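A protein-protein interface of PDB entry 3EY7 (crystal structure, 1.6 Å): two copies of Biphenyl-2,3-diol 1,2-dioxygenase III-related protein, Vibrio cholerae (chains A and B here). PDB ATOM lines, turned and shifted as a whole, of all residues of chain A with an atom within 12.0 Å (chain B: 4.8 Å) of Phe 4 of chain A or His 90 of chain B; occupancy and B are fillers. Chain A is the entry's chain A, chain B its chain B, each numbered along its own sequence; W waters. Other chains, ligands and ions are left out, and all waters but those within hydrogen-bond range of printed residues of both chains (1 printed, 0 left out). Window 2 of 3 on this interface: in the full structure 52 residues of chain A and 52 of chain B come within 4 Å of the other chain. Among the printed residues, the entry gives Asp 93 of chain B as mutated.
O of Lys 30 of chain B lies within hydrogen-bond range of NE2 of His 90 of chain B (2.8 Å). O of Val 31 of chain B lies close to NE2 of His 90 of chain B, at 3.4 Å. The backbone carbonyl oxygen (O) of His 90 of chain B lies within hydrogen-bond range of the side-chain amide nitrogen (NE2) of Gln 94 of chain B (3.0 Å).
Among the printed residues, merely in contact across the chains: Met 6 of chain A with Val 31 of chain B, Met 6 of chain A with His 90 of chain B, Phe 4 of chain A with Asp 86 of chain B, Phe 4 of chain A with Thr 82 of chain B, Phe 4 of chain A with His 90 of chain B, Met 6 of chain A with Ala 87 of chain B and Leu 5 of chain A with Thr 82 of chain B.
Of the printed residues of chain B, Phe 4 of chain A touches Thr 82 (3.7 Å), Asp 86 (3.6 Å) and His 90 (3.7 Å). His 90 of chain B touches just these residues of chain A: Phe 4 and Met 6. Of chain A, only Met 6 (3.4 Å) comes within 4 Å of Val 31 of chain B. Of chain A, only Phe 4 comes within 4 Å of Asp 86 of chain B. No residue of chain A comes within 4 Å of Lys 89 of chain B. Val 91 of chain B touches none of the printed residues of chain A. Asp 93 of chain B touches none of the printed residues of chain A. No residue of chain A comes within 4 Å of Gln 94 of chain B. Of the printed residues of chain B, Met 6 of chain A touches Val 31, Ala 87 and His 90. Of the printed residues of chain B, Leu 5 of chain A touches Thr 82 (3.98 Å). Of the printed residues of chain A, Thr 82 of chain B touches Phe 4 and Leu 5. The nearest printed residue of chain B that does not touch Phe 4 of chain A is Ala 87 of chain B (4.01 Å). The nearest printed residue of chain A that does not touch Thr 82 of chain B is Lys 7 of chain A (4.5 Å).
Of the 9 printed residues of chain A, 3 touch a printed residue of chain B. Printed residues of chain A that touch a printed residue of chain B: Phe 4, Leu 5 and Met 6. Hydrophobic or aromatic side chains of chain B within 4 Å of the printed part of chain A: Ala 87 and His 90. Among the printed residues, 7 pairs touch across the chains. Among the printed residues, no Asp or Glu carboxylate lies within 4 Å of a Lys or Arg side-chain nitrogen of the other chain.
No position is printed for both chains.
Water W1 lies within hydrogen-bond range of a ring nitrogen (ND1) of His 90 of chain B and the backbone carbonyl oxygen (O) of Phe 4 of chain A.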
ATOM      1  N   GLY A   1     -13.995   4.014  22.397  1.00  0.00           N
ATOM      2  CA  GLY A   1     -13.564   3.733  21.038  1.00  0.00           C
ATOM      3  C   GLY A   1     -12.776   4.861  20.411  1.00  0.00           C
ATOM      4  O   GLY A   1     -12.328   5.795  21.086  1.00  0.00           O
ATOM      5  N   MET A   2     -12.613   4.772  19.097  1.00  0.00           N
ATOM      6  CA  MET A   2     -11.841   5.729  18.319  1.00  0.00           C
ATOM      7  C   MET A   2     -12.589   5.945  17.015  1.00  0.00           C
ATOM      8  O   MET A   2     -13.144   5.001  16.470  1.00  0.00           O
ATOM      9  CB  MET A   2     -10.459   5.130  17.991  1.00  0.00           C
ATOM     10  CG  MET A   2      -9.544   5.996  17.134  1.00  0.00           C
ATOM     11  SD  MET A   2      -8.057   4.958  16.341  1.00  0.00           S
ATOM     12  CE  MET A   2      -9.008   4.155  14.854  1.00  0.00           C
ATOM     13  N   GLU A   3     -12.608   7.182  16.523  1.00  0.00           N
ATOM     14  CA  GLU A   3     -13.175   7.515  15.220  1.00  0.00           C
ATOM     15  C   GLU A   3     -14.619   7.066  15.024  1.00  0.00           C
ATOM     16  O   GLU A   3     -14.991   6.576  13.962  1.00  0.00           O
ATOM     17  CB  GLU A   3     -12.267   7.013  14.087  1.00  0.00           C
ATOM     18  CG  GLU A   3     -10.981   7.836  13.943  1.00  0.00           C
ATOM     19  CD  GLU A   3     -11.240   9.248  13.426  1.00  0.00           C
ATOM     20  OE1 GLU A   3     -12.349   9.515  12.891  1.00  0.00           O
ATOM     21  OE2 GLU A   3     -10.335  10.096  13.540  1.00  0.00           O
ATOM     22  N   PHE A   4     -15.451   7.264  16.043  1.00  0.00           N
ATOM     23  CA  PHE A   4     -16.879   7.017  15.888  1.00  0.00           C
ATOM     24  C   PHE A   4     -17.450   7.828  14.715  1.00  0.00           C
ATOM     25  O   PHE A   4     -17.164   9.034  14.569  1.00  0.00           O
ATOM     26  CB  PHE A   4     -17.601   7.412  17.184  1.00  0.00           C
ATOM     27  CG  PHE A   4     -19.107   7.438  17.070  1.00  0.00           C
ATOM     28  CD1 PHE A   4     -19.843   6.272  17.062  1.00  0.00           C
ATOM     29  CD2 PHE A   4     -19.780   8.652  17.017  1.00  0.00           C
ATOM     30  CE1 PHE A   4     -21.246   6.315  16.983  1.00  0.00           C
ATOM     31  CE2 PHE A   4     -21.173   8.698  16.939  1.00  0.00           C
ATOM     32  CZ  PHE A   4     -21.899   7.530  16.912  1.00  0.00           C
ATOM     33  N   LEU A   5     -18.240   7.163  13.874  1.00  0.00           N
ATOM     34  CA  LEU A   5     -18.920   7.815  12.757  1.00  0.00           C
ATOM     35  C   LEU A   5     -20.333   8.179  13.201  1.00  0.00           C
ATOM     36  O   LEU A   5     -21.182   7.297  13.422  1.00  0.00           O
ATOM     37  CB  LEU A   5     -18.994   6.888  11.543  1.00  0.00           C
ATOM     38  CG  LEU A   5     -19.671   7.482  10.306  1.00  0.00           C
ATOM     39  CD1 LEU A   5     -18.718   8.430   9.609  1.00  0.00           C
ATOM     40  CD2 LEU A   5     -20.096   6.362   9.384  1.00  0.00           C
ATOM     41  N   MET A   6     -20.587   9.477  13.309  1.00  0.00           N
ATOM     42  CA  MET A   6     -21.939   9.942  13.574  1.00  0.00           C
ATOM     43  C   MET A   6     -22.767   9.794  12.309  1.00  0.00           C
ATOM     44  O   MET A   6     -22.321  10.144  11.209  1.00  0.00           O
ATOM     45  CB  MET A   6     -21.915  11.407  14.033  1.00  0.00           C
ATOM     46  CG  MET A   6     -23.300  11.975  14.335  1.00  0.00           C
ATOM     47  SD  MET A   6     -24.137  11.002  15.808  1.00  0.00           S
ATOM     48  CE  MET A   6     -25.714  12.144  15.960  1.00  0.00           C
ATOM     49  N   LYS A   7     -23.971   9.260  12.462  1.00  0.00           N
ATOM     50  CA  LYS A   7     -24.831   9.003  11.317  1.00  0.00           C
ATOM     51  C   LYS A   7     -26.296   9.133  11.700  1.00  0.00           C
ATOM     52  O   LYS A   7     -26.753   8.547  12.682  1.00  0.00           O
ATOM     53  CB  LYS A   7     -24.556   7.597  10.793  1.00  0.00           C
ATOM     54  CG  LYS A   7     -25.149   7.273   9.435  1.00  0.00           C
ATOM     55  CD  LYS A   7     -24.723   5.865   9.038  1.00  0.00           C
ATOM     56  CE  LYS A   7     -24.851   5.626   7.546  1.00  0.00           C
ATOM     57  NZ  LYS A   7     -24.373   4.257   7.196  1.00  0.00           N
ATOM     58  N   ILE A   8     -27.035   9.900  10.911  1.00  0.00           N
ATOM     59  CA  ILE A   8     -28.476  10.029  11.104  1.00  0.00           C
ATOM     60  C   ILE A   8     -29.219   9.170  10.076  1.00  0.00           C
ATOM     61  O   ILE A   8     -28.873   9.175   8.900  1.00  0.00           O
ATOM     62  CB  ILE A   8     -28.932  11.503  10.974  1.00  0.00           C
ATOM     63  CG1 ILE A   8     -28.429  12.317  12.175  1.00  0.00           C
ATOM     64  CG2 ILE A   8     -30.438  11.579  10.839  1.00  0.00           C
ATOM     65  CD1 ILE A   8     -28.765  11.678  13.519  1.00  0.00           C
ATOM     66  N   SER A   9     -30.229   8.432  10.537  1.00  0.00           N
ATOM     67  CA  SER A   9     -31.054   7.604   9.657  1.00  0.00           C
ATOM     68  C   SER A   9     -32.116   8.404   8.911  1.00  0.00           C
ATOM     69  O   SER A   9     -32.191   8.349   7.678  1.00  0.00           O
ATOM     70  CB  SER A   9     -31.739   6.485  10.461  1.00  0.00           C
ATOM     71  OG  SER A   9     -32.667   5.789   9.652  1.00  0.00           O
ATOM     72  N   LYS B  30     -20.134  18.156  10.936  1.00  0.00           N
ATOM     73  CA  LYS B  30     -19.344  17.651  12.051  1.00  0.00           C
ATOM     74  C   LYS B  30     -20.190  17.043  13.173  1.00  0.00           C
ATOM     75  O   LYS B  30     -19.880  15.975  13.693  1.00  0.00           O
ATOM     76  CB  LYS B  30     -18.443  18.755  12.614  1.00  0.00           C
ATOM     77  CG  LYS B  30     -17.392  19.244  11.619  1.00  0.00           C
ATOM     78  CD  LYS B  30     -16.644  18.069  10.996  1.00  0.00           C
ATOM     79  CE  LYS B  30     -15.767  18.505   9.829  1.00  0.00           C
ATOM     80  NZ  LYS B  30     -16.566  18.974   8.661  1.00  0.00           N
ATOM     81  N   VAL B  31     -21.266  17.726  13.538  1.00  0.00           N
ATOM     82  CA  VAL B  31     -22.055  17.308  14.696  1.00  0.00           C
ATOM     83  C   VAL B  31     -23.032  16.170  14.373  1.00  0.00           C
ATOM     84  O   VAL B  31     -23.188  15.256  15.168  1.00  0.00           O
ATOM     85  CB  VAL B  31     -22.799  18.504  15.311  1.00  0.00           C
ATOM     86  CG1 VAL B  31     -23.569  18.055  16.545  1.00  0.00           C
ATOM     87  CG2 VAL B  31     -21.813  19.602  15.691  1.00  0.00           C
ATOM     88  N   THR B  82     -27.055   4.428  15.660  1.00  0.00           N
ATOM     89  CA  THR B  82     -25.939   4.258  16.588  1.00  0.00           C
ATOM     90  C   THR B  82     -26.450   4.134  18.036  1.00  0.00           C
ATOM     91  O   THR B  82     -27.595   4.466  18.330  1.00  0.00           O
ATOM     92  CB  THR B  82     -24.904   5.411  16.487  1.00  0.00           C
ATOM     93  OG1 THR B  82     -25.492   6.655  16.919  1.00  0.00           O
ATOM     94  CG2 THR B  82     -24.377   5.578  15.063  1.00  0.00           C
ATOM     95  N   ASP B  86     -23.047   6.786  22.554  1.00  0.00           N
ATOM     96  CA  ASP B  86     -21.984   7.138  21.603  1.00  0.00           C
ATOM     97  C   ASP B  86     -22.319   8.425  20.846  1.00  0.00           C
ATOM     98  O   ASP B  86     -21.463   9.291  20.633  1.00  0.00           O
ATOM     99  CB  ASP B  86     -21.781   6.031  20.572  1.00  0.00           C
ATOM    100  CG  ASP B  86     -21.127   4.790  21.142  1.00  0.00           C
ATOM    101  OD1 ASP B  86     -20.504   4.866  22.223  1.00  0.00           O
ATOM    102  OD2 ASP B  86     -21.229   3.744  20.476  1.00  0.00           O
ATOM    103  N   ALA B  87     -23.573   8.545  20.407  1.00  0.00           N
ATOM    104  CA  ALA B  87     -23.967   9.756  19.694  1.00  0.00           C
ATOM    105  C   ALA B  87     -23.877  10.979  20.622  1.00  0.00           C
ATOM    106  O   ALA B  87     -23.432  12.045  20.201  1.00  0.00           O
ATOM    107  CB  ALA B  87     -25.376   9.600  19.106  1.00  0.00           C
ATOM    108  N   MET B  88     -24.266  10.815  21.883  1.00  0.00           N
ATOM    109  CA  MET B  88     -24.207  11.944  22.804  1.00  0.00           C
ATOM    110  C   MET B  88     -22.764  12.342  23.119  1.00  0.00           C
ATOM    111  O   MET B  88     -22.451  13.526  23.232  1.00  0.00           O
ATOM    112  CB  MET B  88     -24.988  11.654  24.086  1.00  0.00           C
ATOM    113  CG  MET B  88     -25.514  12.903  24.750  1.00  0.00           C
ATOM    114  SD  MET B  88     -26.581  12.512  26.318  1.00  0.00           S
ATOM    115  CE  MET B  88     -25.143  11.831  27.443  1.00  0.00           C
ATOM    116  N   LYS B  89     -21.887  11.351  23.249  1.00  0.00           N
ATOM    117  CA  LYS B  89     -20.470  11.629  23.469  1.00  0.00           C
ATOM    118  C   LYS B  89     -19.897  12.360  22.265  1.00  0.00           C
ATOM    119  O   LYS B  89     -19.116  13.295  22.409  1.00  0.00           O
ATOM    120  CB  LYS B  89     -19.692  10.332  23.718  1.00  0.00           C
ATOM    121  CG  LYS B  89     -18.176  10.494  23.702  1.00  0.00           C
ATOM    122  CD  LYS B  89     -17.501   9.143  23.992  1.00  0.00           C
ATOM    123  CE  LYS B  89     -16.007   9.292  24.258  1.00  0.00           C
ATOM    124  NZ  LYS B  89     -15.251   9.778  23.072  1.00  0.00           N
ATOM    125  N   HIS B  90     -20.291  11.924  21.072  1.00  0.00           N
ATOM    126  CA  HIS B  90     -19.812  12.576  19.869  1.00  0.00           C
ATOM    127  C   HIS B  90     -20.176  14.067  19.858  1.00  0.00           C
ATOM    128  O   HIS B  90     -19.334  14.928  19.583  1.00  0.00           O
ATOM    129  CB  HIS B  90     -20.378  11.903  18.621  1.00  0.00           C
ATOM    130  CG  HIS B  90     -20.086  12.660  17.365  1.00  0.00           C
ATOM    131  ND1 HIS B  90     -18.896  12.531  16.684  1.00  0.00           N
ATOM    132  CD2 HIS B  90     -20.811  13.584  16.686  1.00  0.00           C
ATOM    133  CE1 HIS B  90     -18.908  13.323  15.627  1.00  0.00           C
ATOM    134  NE2 HIS B  90     -20.058  13.975  15.607  1.00  0.00           N
ATOM    135  N   VAL B  91     -21.447  14.360  20.140  1.00  0.00           N
ATOM    136  CA  VAL B  91     -21.966  15.724  20.073  1.00  0.00           C
ATOM    137  C   VAL B  91     -21.268  16.601  21.112  1.00  0.00           C
ATOM    138  O   VAL B  91     -20.784  17.692  20.818  1.00  0.00           O
ATOM    139  CB  VAL B  91     -23.485  15.718  20.283  1.00  0.00           C
ATOM    140  CG1 VAL B  91     -24.014  17.128  20.461  1.00  0.00           C
ATOM    141  CG2 VAL B  91     -24.139  15.040  19.080  1.00  0.00           C
ATOM    142  N   GLU B  92     -21.197  16.075  22.321  1.00  0.00           N
ATOM    143  CA  GLU B  92     -20.520  16.751  23.411  1.00  0.00           C
ATOM    144  C   GLU B  92     -19.057  17.028  23.047  1.00  0.00           C
ATOM    145  O   GLU B  92     -18.522  18.100  23.334  1.00  0.00           O
ATOM    146  CB  GLU B  92     -20.622  15.884  24.656  1.00  0.00           C
ATOM    147  CG  GLU B  92     -20.119  16.528  25.918  1.00  0.00           C
ATOM    148  CD  GLU B  92     -20.056  15.536  27.057  1.00  0.00           C
ATOM    149  OE1 GLU B  92     -19.509  14.428  26.851  1.00  0.00           O
ATOM    150  OE2 GLU B  92     -20.561  15.856  28.148  1.00  0.00           O
ATOM    151  N   ASP B  93     -18.417  16.068  22.389  1.00  0.00           N
ATOM    152  CA  ASP B  93     -17.021  16.241  21.993  1.00  0.00           C
ATOM    153  C   ASP B  93     -16.802  17.254  20.867  1.00  0.00           C
ATOM    154  O   ASP B  93     -15.674  17.692  20.634  1.00  0.00           O
ATOM    155  CB  ASP B  93     -16.377  14.887  21.678  1.00  0.00           C
ATOM    156  CG  ASP B  93     -16.138  14.053  22.937  1.00  0.00           C
ATOM    157  OD1 ASP B  93     -16.386  14.564  24.052  1.00  0.00           O
ATOM    158  OD2 ASP B  93     -15.709  12.891  22.823  1.00  0.00           O
ATOM    159  N   GLN B  94     -17.869  17.646  20.175  1.00  0.00           N
ATOM    160  CA  GLN B  94     -17.753  18.698  19.176  1.00  0.00           C
ATOM    161  C   GLN B  94     -17.937  20.071  19.815  1.00  0.00           C
ATOM    162  O   GLN B  94     -17.984  21.079  19.118  1.00  0.00           O
ATOM    163  CB  GLN B  94     -18.775  18.517  18.042  1.00  0.00           C
ATOM    164  CG  GLN B  94     -18.775  17.147  17.406  1.00  0.00           C
ATOM    165  CD  GLN B  94     -17.379  16.625  17.162  1.00  0.00           C
ATOM    166  OE1 GLN B  94     -16.572  17.267  16.490  1.00  0.00           O
ATOM    167  NE2 GLN B  94     -17.084  15.452  17.709  1.00  0.00           N
HETATM  168  O   HOH W   1     -16.772  10.930  16.783  1.00  0.00           O
